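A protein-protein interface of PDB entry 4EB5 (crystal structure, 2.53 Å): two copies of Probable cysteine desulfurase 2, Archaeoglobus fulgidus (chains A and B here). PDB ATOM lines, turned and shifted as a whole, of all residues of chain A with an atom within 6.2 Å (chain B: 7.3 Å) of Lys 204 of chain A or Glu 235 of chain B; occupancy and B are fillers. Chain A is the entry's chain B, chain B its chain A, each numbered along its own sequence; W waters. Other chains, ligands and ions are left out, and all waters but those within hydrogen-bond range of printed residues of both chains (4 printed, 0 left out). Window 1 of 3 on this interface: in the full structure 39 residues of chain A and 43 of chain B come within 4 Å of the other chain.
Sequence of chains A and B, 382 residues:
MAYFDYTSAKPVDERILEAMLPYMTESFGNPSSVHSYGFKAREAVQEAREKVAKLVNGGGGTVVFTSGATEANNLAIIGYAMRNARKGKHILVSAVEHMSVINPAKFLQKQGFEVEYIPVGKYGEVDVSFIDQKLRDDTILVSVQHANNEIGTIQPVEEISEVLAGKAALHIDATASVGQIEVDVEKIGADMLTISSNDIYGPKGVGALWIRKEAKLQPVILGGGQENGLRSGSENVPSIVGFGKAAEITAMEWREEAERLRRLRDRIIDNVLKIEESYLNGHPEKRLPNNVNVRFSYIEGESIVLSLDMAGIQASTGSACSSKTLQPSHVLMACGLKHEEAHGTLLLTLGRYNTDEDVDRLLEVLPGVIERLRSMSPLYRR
Water W1 bridges the backbone carbonyl oxygen of Glu 235 of chain B and the side-chain amino group of Lys 204 of chain A. Water W4 lies within hydrogen-bond range of O of Ser 8 of chain A (2.6 Å) and ND2 of Asn 30 of chain B (3.4 Å). Water W3 lies within hydrogen-bond range of O of Tyr 23 of chain B (2.6 Å) and NZ of Lys 204 of chain A (2.9 Å). Water W2 bridges OG of Ser 67 of chain A (3.0 Å) and NH1 of Arg 231 of chain B (3.4 Å).
Phe 28 of chain B touches Ala 9 of chain A (O to CB, 3.2 Å). Gly 29 of chain B touches Ala 9 of chain A (C to CB, 3.9 Å). CB of Ala 9 of chain A touches N of Asn 30 of chain B, 3.7 Å away. Lys 10 of chain A touches Phe 28 of chain B. O of Glu 235 of chain B touches CD of Lys 204 of chain A, 3.9 Å away. Lys 204 of chain A touches Asn 236 of chain B (CB to OD1, 3.7 Å). Gly 205 of chain A touches Asn 236 of chain B (CA to ND2, 3.3 Å). Gly 205 of chain B touches Asn 236 of chain A.
Printed residues of chain A that touch a printed residue of chain B: Ser 8, Ala 9, Lys 10, Val 12, Ser 67, Lys 204, Gly 205 and Asn 236. Hydrophobic or aromatic side chains of chain A that line the printed part of chain B: Ala 9 and Val 12. Of the 26 printed residues of chain B, 8 touch a printed residue of chain A. Printed residues of chain B that touch a printed residue of chain A: Met 24, Phe 28, Gly 29, Asn 30, Gly 205, Arg 231, Glu 235 and Asn 236. Among the printed residues, 13 pairs touch across the chains.
The side-chain hydroxyl (OG) of Ser 67 of chain A lies within hydrogen-bond range of the guanidinium group (NH2) of Arg 231 of chain B (2.9 Å). O of Met 24 of chain B is in hydrogen-bond range of N of Val 12 of chain A (3.0 Å). O of Phe 28 of chain B is in hydrogen-bond range of NZ of Lys 204 of chain A, at 3.0 Å. The backbone carbonyl oxygen (O) of Ser 8 of chain A sits at hydrogen-bond distance from the side-chain amide nitrogen (ND2) of Asn 30 of chain B (2.7 Å). NZ of Lys 204 of chain A sits at hydrogen-bond distance from O of Gly 29 of chain B.
Of the printed residues of chain B, Lys 204 of chain A touches Phe 28, Gly 29, Glu 235 and Asn 236. Glu 235 of chain B touches one residue of chain A. Of the printed residues of chain B, Gly 205 of chain A touches Asn 236. Of the printed residues of chain A, Gly 29 of chain B touches Ala 9 (3.9 Å) and Lys 204 (3.4 Å). Printed residues of chain B within 4 Å of Ala 9 of chain A: Phe 28, Gly 29 and Asn 30. The nearest printed residue of chain A that does not touch Glu 235 of chain B is Gly 205 of chain A (6.5 Å).
The side-chain amide nitrogen (ND2) of Asn 236 of chain A lies within hydrogen-bond range of the side-chain hydroxyl (OG) of Ser 239 of chain A. N of Lys 10 of chain A sits at hydrogen-bond distance from OD1 of Asn 198 of chain A (3.0 Å). The side-chain amide oxygen (OD1) of Asn 30 of chain B is in hydrogen-bond range of the backbone NH (N) of Ser 32 of chain B, 3.0 Å away. The backbone NH of Arg 231 of chain B lies close to the backbone carbonyl oxygen of Gln 226 of chain B. ND2 of Asn 236 of chain B is in hydrogen-bond range of OG of Ser 239 of chain B (2.7 Å).
Gly 205 of chain A touches Asn 236 of chain B, and with the chains exchanged Asn 236 of chain A touches Gly 205 of chain B. Positions printed for both chains: 205, 236 and 239.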
ATOM      1  N   SER A   8     -23.957   0.199 -27.009  1.00  0.00           N
ATOM      2  CA  SER A   8     -23.510   0.062 -25.630  1.00  0.00           C
ATOM      3  C   SER A   8     -22.034   0.385 -25.418  1.00  0.00           C
ATOM      4  O   SER A   8     -21.632   0.808 -24.337  1.00  0.00           O
ATOM      5  CB  SER A   8     -23.854  -1.319 -25.107  1.00  0.00           C
ATOM      6  OG  SER A   8     -25.261  -1.368 -24.974  1.00  0.00           O
ATOM      7  N   ALA A   9     -21.241   0.206 -26.467  1.00  0.00           N
ATOM      8  CA  ALA A   9     -19.802   0.291 -26.364  1.00  0.00           C
ATOM      9  C   ALA A   9     -19.262   0.066 -27.744  1.00  0.00           C
ATOM     10  O   ALA A   9     -19.861  -0.670 -28.524  1.00  0.00           O
ATOM     11  CB  ALA A   9     -19.259  -0.795 -25.418  1.00  0.00           C
ATOM     12  N   LYS A  10     -18.125   0.679 -28.035  1.00  0.00           N
ATOM     13  CA  LYS A  10     -17.458   0.521 -29.314  1.00  0.00           C
ATOM     14  C   LYS A  10     -15.972   0.377 -29.051  1.00  0.00           C
ATOM     15  O   LYS A  10     -15.455   1.002 -28.135  1.00  0.00           O
ATOM     16  CB  LYS A  10     -17.651   1.760 -30.187  1.00  0.00           C
ATOM     17  CG  LYS A  10     -19.040   1.957 -30.741  1.00  0.00           C
ATOM     18  CD  LYS A  10     -19.018   3.017 -31.844  1.00  0.00           C
ATOM     19  CE  LYS A  10     -20.372   3.211 -32.474  1.00  0.00           C
ATOM     20  NZ  LYS A  10     -21.489   3.283 -31.508  1.00  0.00           N
ATOM     21  N   VAL A  12     -12.088   1.251 -29.772  1.00  0.00           N
ATOM     22  CA  VAL A  12     -11.316   2.383 -30.279  1.00  0.00           C
ATOM     23  C   VAL A  12     -10.596   1.946 -31.551  1.00  0.00           C
ATOM     24  O   VAL A  12      -9.993   0.876 -31.592  1.00  0.00           O
ATOM     25  CB  VAL A  12     -10.269   2.825 -29.229  1.00  0.00           C
ATOM     26  CG1 VAL A  12      -9.567   4.073 -29.675  1.00  0.00           C
ATOM     27  CG2 VAL A  12     -10.953   3.006 -27.873  1.00  0.00           C
ATOM     28  N   SER A  67     -16.209  14.510 -19.493  1.00  0.00           N
ATOM     29  CA  SER A  67     -15.903  13.107 -19.280  1.00  0.00           C
ATOM     30  C   SER A  67     -16.860  12.181 -20.022  1.00  0.00           C
ATOM     31  O   SER A  67     -16.757  10.979 -19.921  1.00  0.00           O
ATOM     32  CB  SER A  67     -15.920  12.791 -17.798  1.00  0.00           C
ATOM     33  OG  SER A  67     -17.252  12.711 -17.307  1.00  0.00           O
ATOM     34  N   SER A 197     -17.383  10.769 -27.612  1.00  0.00           N
ATOM     35  CA  SER A 197     -16.182  10.213 -28.248  1.00  0.00           C
ATOM     36  C   SER A 197     -16.221   8.724 -28.591  1.00  0.00           C
ATOM     37  O   SER A 197     -15.696   8.317 -29.625  1.00  0.00           O
ATOM     38  CB  SER A 197     -14.948  10.522 -27.399  1.00  0.00           C
ATOM     39  OG  SER A 197     -13.924   9.621 -27.695  1.00  0.00           O
ATOM     40  N   ASN A 198     -16.820   7.901 -27.741  1.00  0.00           N
ATOM     41  CA  ASN A 198     -16.825   6.480 -28.042  1.00  0.00           C
ATOM     42  C   ASN A 198     -17.823   6.115 -29.130  1.00  0.00           C
ATOM     43  O   ASN A 198     -17.691   5.083 -29.796  1.00  0.00           O
ATOM     44  CB  ASN A 198     -17.109   5.669 -26.794  1.00  0.00           C
ATOM     45  CG  ASN A 198     -16.834   4.200 -26.978  1.00  0.00           C
ATOM     46  OD1 ASN A 198     -17.743   3.373 -26.849  1.00  0.00           O
ATOM     47  ND2 ASN A 198     -15.583   3.857 -27.283  1.00  0.00           N
ATOM     48  N   GLY A 202     -13.752   6.943 -30.866  1.00  0.00           N
ATOM     49  CA  GLY A 202     -12.727   7.564 -30.059  1.00  0.00           C
ATOM     50  C   GLY A 202     -12.688   6.745 -28.790  1.00  0.00           C
ATOM     51  O   GLY A 202     -13.445   5.783 -28.649  1.00  0.00           O
ATOM     52  N   PRO A 203     -11.809   7.108 -27.864  1.00  0.00           N
ATOM     53  CA  PRO A 203     -11.727   6.441 -26.561  1.00  0.00           C
ATOM     54  C   PRO A 203     -12.929   6.772 -25.721  1.00  0.00           C
ATOM     55  O   PRO A 203     -13.508   7.823 -25.899  1.00  0.00           O
ATOM     56  CB  PRO A 203     -10.527   7.092 -25.902  1.00  0.00           C
ATOM     57  CG  PRO A 203     -10.459   8.470 -26.577  1.00  0.00           C
ATOM     58  CD  PRO A 203     -10.960   8.303 -27.966  1.00  0.00           C
ATOM     59  N   LYS A 204     -13.298   5.867 -24.821  1.00  0.00           N
ATOM     60  CA  LYS A 204     -14.266   6.149 -23.755  1.00  0.00           C
ATOM     61  C   LYS A 204     -13.672   7.165 -22.764  1.00  0.00           C
ATOM     62  O   LYS A 204     -12.465   7.378 -22.729  1.00  0.00           O
ATOM     63  CB  LYS A 204     -14.600   4.861 -22.993  1.00  0.00           C
ATOM     64  CG  LYS A 204     -15.093   3.694 -23.845  1.00  0.00           C
ATOM     65  CD  LYS A 204     -15.466   2.482 -22.990  1.00  0.00           C
ATOM     66  CE  LYS A 204     -15.741   1.225 -23.821  1.00  0.00           C
ATOM     67  NZ  LYS A 204     -16.224   0.155 -22.888  1.00  0.00           N
ATOM     68  N   GLY A 205     -14.492   7.777 -21.938  1.00  0.00           N
ATOM     69  CA  GLY A 205     -13.940   8.601 -20.882  1.00  0.00           C
ATOM     70  C   GLY A 205     -13.923  10.086 -21.196  1.00  0.00           C
ATOM     71  O   GLY A 205     -13.672  10.885 -20.321  1.00  0.00           O
ATOM     72  N   VAL A 206     -14.203  10.455 -22.445  1.00  0.00           N
ATOM     73  CA  VAL A 206     -14.195  11.863 -22.834  1.00  0.00           C
ATOM     74  C   VAL A 206     -15.412  12.213 -23.707  1.00  0.00           C
ATOM     75  O   VAL A 206     -15.955  11.361 -24.393  1.00  0.00           O
ATOM     76  CB  VAL A 206     -12.828  12.245 -23.516  1.00  0.00           C
ATOM     77  CG1 VAL A 206     -12.578  11.403 -24.754  1.00  0.00           C
ATOM     78  CG2 VAL A 206     -12.757  13.715 -23.840  1.00  0.00           C
ATOM     79  N   ASN A 236      -7.520  15.686 -19.715  1.00  0.00           N
ATOM     80  CA  ASN A 236      -7.095  14.323 -20.059  1.00  0.00           C
ATOM     81  C   ASN A 236      -6.641  14.315 -21.521  1.00  0.00           C
ATOM     82  O   ASN A 236      -7.347  13.852 -22.423  1.00  0.00           O
ATOM     83  CB  ASN A 236      -8.236  13.350 -19.749  1.00  0.00           C
ATOM     84  CG  ASN A 236      -7.987  11.913 -20.214  1.00  0.00           C
ATOM     85  OD1 ASN A 236      -6.862  11.468 -20.540  1.00  0.00           O
ATOM     86  ND2 ASN A 236      -9.077  11.173 -20.255  1.00  0.00           N
ATOM     87  N   SER A 239      -6.853  11.369 -24.086  1.00  0.00           N
ATOM     88  CA  SER A 239      -8.206  11.042 -24.559  1.00  0.00           C
ATOM     89  C   SER A 239      -8.818  12.106 -25.456  1.00  0.00           C
ATOM     90  O   SER A 239      -9.644  11.823 -26.334  1.00  0.00           O
ATOM     91  CB  SER A 239      -9.135  10.828 -23.359  1.00  0.00           C
ATOM     92  OG  SER A 239      -8.870   9.599 -22.702  1.00  0.00           O
ATOM     93  N   TYR B  23      -8.438  -3.734 -23.151  1.00  0.00           N
ATOM     94  CA  TYR B  23      -9.814  -3.284 -22.994  1.00  0.00           C
ATOM     95  C   TYR B  23     -10.263  -2.205 -24.008  1.00  0.00           C
ATOM     96  O   TYR B  23     -11.455  -1.933 -24.151  1.00  0.00           O
ATOM     97  CB  TYR B  23     -10.091  -2.918 -21.537  1.00  0.00           C
ATOM     98  CG  TYR B  23      -9.962  -4.137 -20.662  1.00  0.00           C
ATOM     99  CD1 TYR B  23     -11.081  -4.912 -20.357  1.00  0.00           C
ATOM    100  CD2 TYR B  23      -8.708  -4.563 -20.194  1.00  0.00           C
ATOM    101  CE1 TYR B  23     -10.963  -6.056 -19.583  1.00  0.00           C
ATOM    102  CE2 TYR B  23      -8.589  -5.700 -19.404  1.00  0.00           C
ATOM    103  CZ  TYR B  23      -9.721  -6.437 -19.115  1.00  0.00           C
ATOM    104  OH  TYR B  23      -9.640  -7.553 -18.347  1.00  0.00           O
ATOM    105  N   MET B  24      -9.299  -1.649 -24.737  1.00  0.00           N
ATOM    106  CA  MET B  24      -9.552  -0.600 -25.697  1.00  0.00           C
ATOM    107  C   MET B  24      -9.897  -1.082 -27.092  1.00  0.00           C
ATOM    108  O   MET B  24     -10.570  -0.384 -27.839  1.00  0.00           O
ATOM    109  CB  MET B  24      -8.351   0.332 -25.762  1.00  0.00           C
ATOM    110  CG  MET B  24      -8.231   1.165 -24.505  1.00  0.00           C
ATOM    111  SD  MET B  24      -7.396   2.707 -24.812  1.00  0.00           S
ATOM    112  CE  MET B  24      -5.754   2.368 -24.179  1.00  0.00           C
ATOM    113  N   SER B  27     -11.348  -6.287 -25.732  1.00  0.00           N
ATOM    114  CA  SER B  27     -12.460  -6.513 -24.828  1.00  0.00           C
ATOM    115  C   SER B  27     -13.175  -5.233 -24.397  1.00  0.00           C
ATOM    116  O   SER B  27     -13.179  -4.870 -23.223  1.00  0.00           O
ATOM    117  CB  SER B  27     -12.021  -7.339 -23.626  1.00  0.00           C
ATOM    118  OG  SER B  27     -13.199  -7.872 -23.058  1.00  0.00           O
ATOM    119  N   PHE B  28     -13.831  -4.593 -25.353  1.00  0.00           N
ATOM    120  CA  PHE B  28     -14.403  -3.259 -25.183  1.00  0.00           C
ATOM    121  C   PHE B  28     -15.859  -3.241 -24.650  1.00  0.00           C
ATOM    122  O   PHE B  28     -16.507  -2.192 -24.677  1.00  0.00           O
ATOM    123  CB  PHE B  28     -14.360  -2.548 -26.529  1.00  0.00           C
ATOM    124  CG  PHE B  28     -14.982  -3.361 -27.640  1.00  0.00           C
ATOM    125  CD1 PHE B  28     -16.332  -3.223 -27.950  1.00  0.00           C
ATOM    126  CD2 PHE B  28     -14.205  -4.285 -28.372  1.00  0.00           C
ATOM    127  CE1 PHE B  28     -16.909  -3.990 -28.962  1.00  0.00           C
ATOM    128  CE2 PHE B  28     -14.761  -5.046 -29.378  1.00  0.00           C
ATOM    129  CZ  PHE B  28     -16.129  -4.907 -29.681  1.00  0.00           C
ATOM    130  N   GLY B  29     -16.392  -4.363 -24.194  1.00  0.00           N
ATOM    131  CA  GLY B  29     -17.786  -4.363 -23.765  1.00  0.00           C
ATOM    132  C   GLY B  29     -18.199  -3.387 -22.653  1.00  0.00           C
ATOM    133  O   GLY B  29     -17.384  -2.854 -21.906  1.00  0.00           O
ATOM    134  N   ASN B  30     -19.499  -3.170 -22.565  1.00  0.00           N
ATOM    135  CA  ASN B  30     -20.136  -2.350 -21.559  1.00  0.00           C
ATOM    136  C   ASN B  30     -20.551  -3.213 -20.370  1.00  0.00           C
ATOM    137  O   ASN B  30     -21.317  -4.151 -20.515  1.00  0.00           O
ATOM    138  CB  ASN B  30     -21.351  -1.677 -22.169  1.00  0.00           C
ATOM    139  CG  ASN B  30     -22.002  -0.670 -21.239  1.00  0.00           C
ATOM    140  OD1 ASN B  30     -22.088  -0.867 -20.002  1.00  0.00           O
ATOM    141  ND2 ASN B  30     -22.527   0.411 -21.840  1.00  0.00           N
ATOM    142  N   PRO B  31     -20.033  -2.892 -19.178  1.00  0.00           N
ATOM    143  CA  PRO B  31     -20.341  -3.602 -17.916  1.00  0.00           C
ATOM    144  C   PRO B  31     -21.834  -3.928 -17.660  1.00  0.00           C
ATOM    145  O   PRO B  31     -22.117  -4.962 -17.087  1.00  0.00           O
ATOM    146  CB  PRO B  31     -19.790  -2.665 -16.829  1.00  0.00           C
ATOM    147  CG  PRO B  31     -19.353  -1.435 -17.530  1.00  0.00           C
ATOM    148  CD  PRO B  31     -19.140  -1.746 -18.967  1.00  0.00           C
ATOM    149  N   SER B  32     -22.751  -3.067 -18.095  1.00  0.00           N
ATOM    150  CA  SER B  32     -24.189  -3.313 -18.037  1.00  0.00           C
ATOM    151  C   SER B  32     -24.760  -4.210 -19.149  1.00  0.00           C
ATOM    152  O   SER B  32     -25.921  -4.618 -19.073  1.00  0.00           O
ATOM    153  CB  SER B  32     -24.943  -1.984 -18.078  1.00  0.00           C
ATOM    154  OG  SER B  32     -24.752  -1.230 -16.874  1.00  0.00           O
ATOM    155  N   ALA B  41     -16.445  -7.363 -18.783  1.00  0.00           N
ATOM    156  CA  ALA B  41     -16.329  -5.932 -18.454  1.00  0.00           C
ATOM    157  C   ALA B  41     -16.597  -5.658 -16.990  1.00  0.00           C
ATOM    158  O   ALA B  41     -15.861  -4.897 -16.350  1.00  0.00           O
ATOM    159  CB  ALA B  41     -17.262  -5.069 -19.325  1.00  0.00           C
ATOM    160  N   ARG B  42     -17.656  -6.275 -16.476  1.00  0.00           N
ATOM    161  CA  ARG B  42     -17.998  -6.175 -15.079  1.00  0.00           C
ATOM    162  C   ARG B  42     -16.858  -6.731 -14.235  1.00  0.00           C
ATOM    163  O   ARG B  42     -16.417  -6.112 -13.291  1.00  0.00           O
ATOM    164  CB  ARG B  42     -19.295  -6.951 -14.793  1.00  0.00           C
ATOM    165  CG  ARG B  42     -20.471  -6.081 -14.342  1.00  0.00           C
ATOM    166  CD  ARG B  42     -21.780  -6.887 -14.285  1.00  0.00           C
ATOM    167  N   VAL B  45     -13.915  -4.481 -14.010  1.00  0.00           N
ATOM    168  CA  VAL B  45     -14.236  -3.275 -13.219  1.00  0.00           C
ATOM    169  C   VAL B  45     -14.178  -3.592 -11.741  1.00  0.00           C
ATOM    170  O   VAL B  45     -13.599  -2.805 -10.972  1.00  0.00           O
ATOM    171  CB  VAL B  45     -15.576  -2.610 -13.570  1.00  0.00           C
ATOM    172  CG1 VAL B  45     -15.888  -1.509 -12.579  1.00  0.00           C
ATOM    173  CG2 VAL B  45     -15.517  -2.000 -14.912  1.00  0.00           C
ATOM    174  N   ARG B  49     -11.900  -2.390  -8.610  1.00  0.00           N
ATOM    175  CA  ARG B  49     -12.550  -1.743  -7.478  1.00  0.00           C
ATOM    176  C   ARG B  49     -11.927  -2.271  -6.182  1.00  0.00           C
ATOM    177  O   ARG B  49     -11.601  -1.514  -5.267  1.00  0.00           O
ATOM    178  CB  ARG B  49     -14.059  -1.982  -7.530  1.00  0.00           C
ATOM    179  CG  ARG B  49     -14.867  -1.060  -6.638  1.00  0.00           C
ATOM    180  CD  ARG B  49     -16.373  -1.316  -6.642  1.00  0.00           C
ATOM    181  NE  ARG B  49     -16.942  -1.253  -7.998  1.00  0.00           N
ATOM    182  CZ  ARG B  49     -17.148  -0.139  -8.704  1.00  0.00           C
ATOM    183  NH1 ARG B  49     -16.852   1.049  -8.201  1.00  0.00           N
ATOM    184  NH2 ARG B  49     -17.628  -0.211  -9.934  1.00  0.00           N
ATOM    185  N   PHE B  65     -15.987   5.274  -8.823  1.00  0.00           N
ATOM    186  CA  PHE B  65     -15.042   5.786  -9.816  1.00  0.00           C
ATOM    187  C   PHE B  65     -15.552   7.138 -10.368  1.00  0.00           C
ATOM    188  O   PHE B  65     -16.759   7.343 -10.520  1.00  0.00           O
ATOM    189  CB  PHE B  65     -14.750   4.752 -10.942  1.00  0.00           C
ATOM    190  CG  PHE B  65     -13.973   3.514 -10.470  1.00  0.00           C
ATOM    191  CD1 PHE B  65     -12.640   3.611 -10.033  1.00  0.00           C
ATOM    192  CD2 PHE B  65     -14.567   2.261 -10.467  1.00  0.00           C
ATOM    193  CE1 PHE B  65     -11.923   2.479  -9.597  1.00  0.00           C
ATOM    194  CE2 PHE B  65     -13.855   1.118 -10.046  1.00  0.00           C
ATOM    195  CZ  PHE B  65     -12.525   1.233  -9.615  1.00  0.00           C
ATOM    196  N   GLY B 205      -7.720  11.143 -16.298  1.00  0.00           N
ATOM    197  CA  GLY B 205      -9.139  11.067 -16.648  1.00  0.00           C
ATOM    198  C   GLY B 205      -9.945  10.021 -15.899  1.00  0.00           C
ATOM    199  O   GLY B 205     -11.024   9.625 -16.340  1.00  0.00           O
ATOM    200  N   GLN B 226     -25.509   4.082 -12.936  1.00  0.00           N
ATOM    201  CA  GLN B 226     -24.219   3.429 -12.706  1.00  0.00           C
ATOM    202  C   GLN B 226     -23.617   3.874 -11.379  1.00  0.00           C
ATOM    203  O   GLN B 226     -23.961   4.948 -10.873  1.00  0.00           O
ATOM    204  CB  GLN B 226     -23.202   3.753 -13.807  1.00  0.00           C
ATOM    205  CG  GLN B 226     -23.558   3.280 -15.196  1.00  0.00           C
ATOM    206  CD  GLN B 226     -24.406   4.277 -15.947  1.00  0.00           C
ATOM    207  OE1 GLN B 226     -25.070   5.128 -15.355  1.00  0.00           O
ATOM    208  NE2 GLN B 226     -24.391   4.179 -17.256  1.00  0.00           N
ATOM    209  N   GLU B 227     -22.685   3.054 -10.869  1.00  0.00           N
ATOM    210  CA  GLU B 227     -22.043   3.205  -9.563  1.00  0.00           C
ATOM    211  C   GLU B 227     -23.081   3.253  -8.452  1.00  0.00           C
ATOM    212  O   GLU B 227     -22.967   4.027  -7.509  1.00  0.00           O
ATOM    213  CB  GLU B 227     -21.128   4.438  -9.531  1.00  0.00           C
ATOM    214  CG  GLU B 227     -19.919   4.402 -10.516  1.00  0.00           C
ATOM    215  CD  GLU B 227     -18.910   3.277 -10.209  1.00  0.00           C
ATOM    216  OE1 GLU B 227     -18.802   2.890  -9.024  1.00  0.00           O
ATOM    217  OE2 GLU B 227     -18.233   2.786 -11.151  1.00  0.00           O
ATOM    218  N   ARG B 231     -22.910   7.867  -9.384  1.00  0.00           N
ATOM    219  CA  ARG B 231     -22.190   8.516 -10.482  1.00  0.00           C
ATOM    220  C   ARG B 231     -22.498   7.867 -11.818  1.00  0.00           C
ATOM    221  O   ARG B 231     -21.817   6.918 -12.193  1.00  0.00           O
ATOM    222  CB  ARG B 231     -20.672   8.450 -10.256  1.00  0.00           C
ATOM    223  CG  ARG B 231     -19.836   9.468 -11.046  1.00  0.00           C
ATOM    224  CD  ARG B 231     -19.677   9.176 -12.543  1.00  0.00           C
ATOM    225  NE  ARG B 231     -18.811  10.192 -13.145  1.00  0.00           N
ATOM    226  CZ  ARG B 231     -18.854  10.628 -14.405  1.00  0.00           C
ATOM    227  NH1 ARG B 231     -19.753  10.164 -15.271  1.00  0.00           N
ATOM    228  NH2 ARG B 231     -18.005  11.575 -14.770  1.00  0.00           N
ATOM    229  N   SER B 232     -23.490   8.405 -12.532  1.00  0.00           N
ATOM    230  CA  SER B 232     -23.941   7.934 -13.862  1.00  0.00           C
ATOM    231  C   SER B 232     -22.955   8.069 -15.037  1.00  0.00           C
ATOM    232  O   SER B 232     -22.063   8.928 -15.003  1.00  0.00           O
ATOM    233  CB  SER B 232     -25.234   8.651 -14.230  1.00  0.00           C
ATOM    234  OG  SER B 232     -26.298   8.021 -13.577  1.00  0.00           O
ATOM    235  N   GLY B 233     -23.151   7.241 -16.076  1.00  0.00           N
ATOM    236  CA  GLY B 233     -22.251   7.197 -17.250  1.00  0.00           C
ATOM    237  C   GLY B 233     -21.624   5.818 -17.532  1.00  0.00           C
ATOM    238  O   GLY B 233     -20.971   5.230 -16.683  1.00  0.00           O
ATOM    239  N   SER B 234     -21.810   5.305 -18.744  1.00  0.00           N
ATOM    240  CA  SER B 234     -21.127   4.091 -19.179  1.00  0.00           C
ATOM    241  C   SER B 234     -19.706   4.105 -18.643  1.00  0.00           C
ATOM    242  O   SER B 234     -19.032   5.141 -18.686  1.00  0.00           O
ATOM    243  CB  SER B 234     -21.069   4.033 -20.706  1.00  0.00           C
ATOM    244  OG  SER B 234     -22.344   4.141 -21.290  1.00  0.00           O
ATOM    245  N   GLU B 235     -19.240   2.965 -18.152  1.00  0.00           N
ATOM    246  CA  GLU B 235     -17.993   2.942 -17.406  1.00  0.00           C
ATOM    247  C   GLU B 235     -16.788   2.928 -18.329  1.00  0.00           C
ATOM    248  O   GLU B 235     -16.792   2.273 -19.376  1.00  0.00           O
ATOM    249  CB  GLU B 235     -17.977   1.770 -16.432  1.00  0.00           C
ATOM    250  CG  GLU B 235     -19.058   1.870 -15.288  1.00  0.00           C
ATOM    251  CD  GLU B 235     -20.325   1.066 -15.590  1.00  0.00           C
ATOM    252  OE1 GLU B 235     -20.944   1.288 -16.671  1.00  0.00           O
ATOM    253  OE2 GLU B 235     -20.704   0.195 -14.762  1.00  0.00           O
ATOM    254  N   ASN B 236     -15.778   3.706 -17.958  1.00  0.00           N
ATOM    255  CA  ASN B 236     -14.568   3.824 -18.704  1.00  0.00           C
ATOM    256  C   ASN B 236     -13.705   2.661 -18.259  1.00  0.00           C
ATOM    257  O   ASN B 236     -12.736   2.822 -17.527  1.00  0.00           O
ATOM    258  CB  ASN B 236     -13.921   5.175 -18.416  1.00  0.00           C
ATOM    259  CG  ASN B 236     -12.671   5.444 -19.277  1.00  0.00           C
ATOM    260  OD1 ASN B 236     -12.272   4.636 -20.120  1.00  0.00           O
ATOM    261  ND2 ASN B 236     -12.051   6.580 -19.044  1.00  0.00           N
ATOM    262  N   VAL B 237     -14.083   1.476 -18.729  1.00  0.00           N
ATOM    263  CA  VAL B 237     -13.451   0.253 -18.332  1.00  0.00           C
ATOM    264  C   VAL B 237     -11.932   0.280 -18.462  1.00  0.00           C
ATOM    265  O   VAL B 237     -11.255  -0.150 -17.526  1.00  0.00           O
ATOM    266  CB  VAL B 237     -14.044  -0.979 -19.067  1.00  0.00           C
ATOM    267  CG1 VAL B 237     -13.336  -2.245 -18.627  1.00  0.00           C
ATOM    268  CG2 VAL B 237     -15.578  -1.069 -18.834  1.00  0.00           C
ATOM    269  N   PRO B 238     -11.381   0.780 -19.596  1.00  0.00           N
ATOM    270  CA  PRO B 238      -9.905   0.699 -19.676  1.00  0.00           C
ATOM    271  C   PRO B 238      -9.180   1.539 -18.632  1.00  0.00           C
ATOM    272  O   PRO B 238      -8.097   1.131 -18.156  1.00  0.00           O
ATOM    273  CB  PRO B 238      -9.595   1.192 -21.099  1.00  0.00           C
ATOM    274  CG  PRO B 238     -10.937   0.966 -21.863  1.00  0.00           C
ATOM    275  CD  PRO B 238     -11.967   1.325 -20.840  1.00  0.00           C
ATOM    276  N   SER B 239      -9.760   2.684 -18.246  1.00  0.00           N
ATOM    277  CA  SER B 239      -9.031   3.594 -17.337  1.00  0.00           C
ATOM    278  C   SER B 239      -9.069   3.002 -15.971  1.00  0.00           C
ATOM    279  O   SER B 239      -8.069   3.099 -15.221  1.00  0.00           O
ATOM    280  CB  SER B 239      -9.621   4.992 -17.281  1.00  0.00           C
ATOM    281  OG  SER B 239      -9.578   5.598 -18.559  1.00  0.00           O
ATOM    282  N   ILE B 240     -10.214   2.370 -15.678  1.00  0.00           N
ATOM    283  CA  ILE B 240     -10.489   1.748 -14.394  1.00  0.00           C
ATOM    284  C   ILE B 240      -9.491   0.603 -14.207  1.00  0.00           C
ATOM    285  O   ILE B 240      -8.764   0.577 -13.216  1.00  0.00           O
ATOM    286  CB  ILE B 240     -12.018   1.353 -14.239  1.00  0.00           C
ATOM    287  CG1 ILE B 240     -12.890   2.636 -14.027  1.00  0.00           C
ATOM    288  CG2 ILE B 240     -12.230   0.335 -13.139  1.00  0.00           C
ATOM    289  CD1 ILE B 240     -14.408   2.549 -14.502  1.00  0.00           C
HETATM  290  O   HOH W   1     -18.129   0.817 -20.991  1.00  0.00           O
HETATM  291  O   HOH W   2     -19.861  11.615 -18.296  1.00  0.00           O
HETATM  292  O   HOH W   3     -13.531  -0.811 -23.069  1.00  0.00           O
HETATM  293  O   HOH W   4     -19.818   2.108 -23.073  1.00  0.00           O
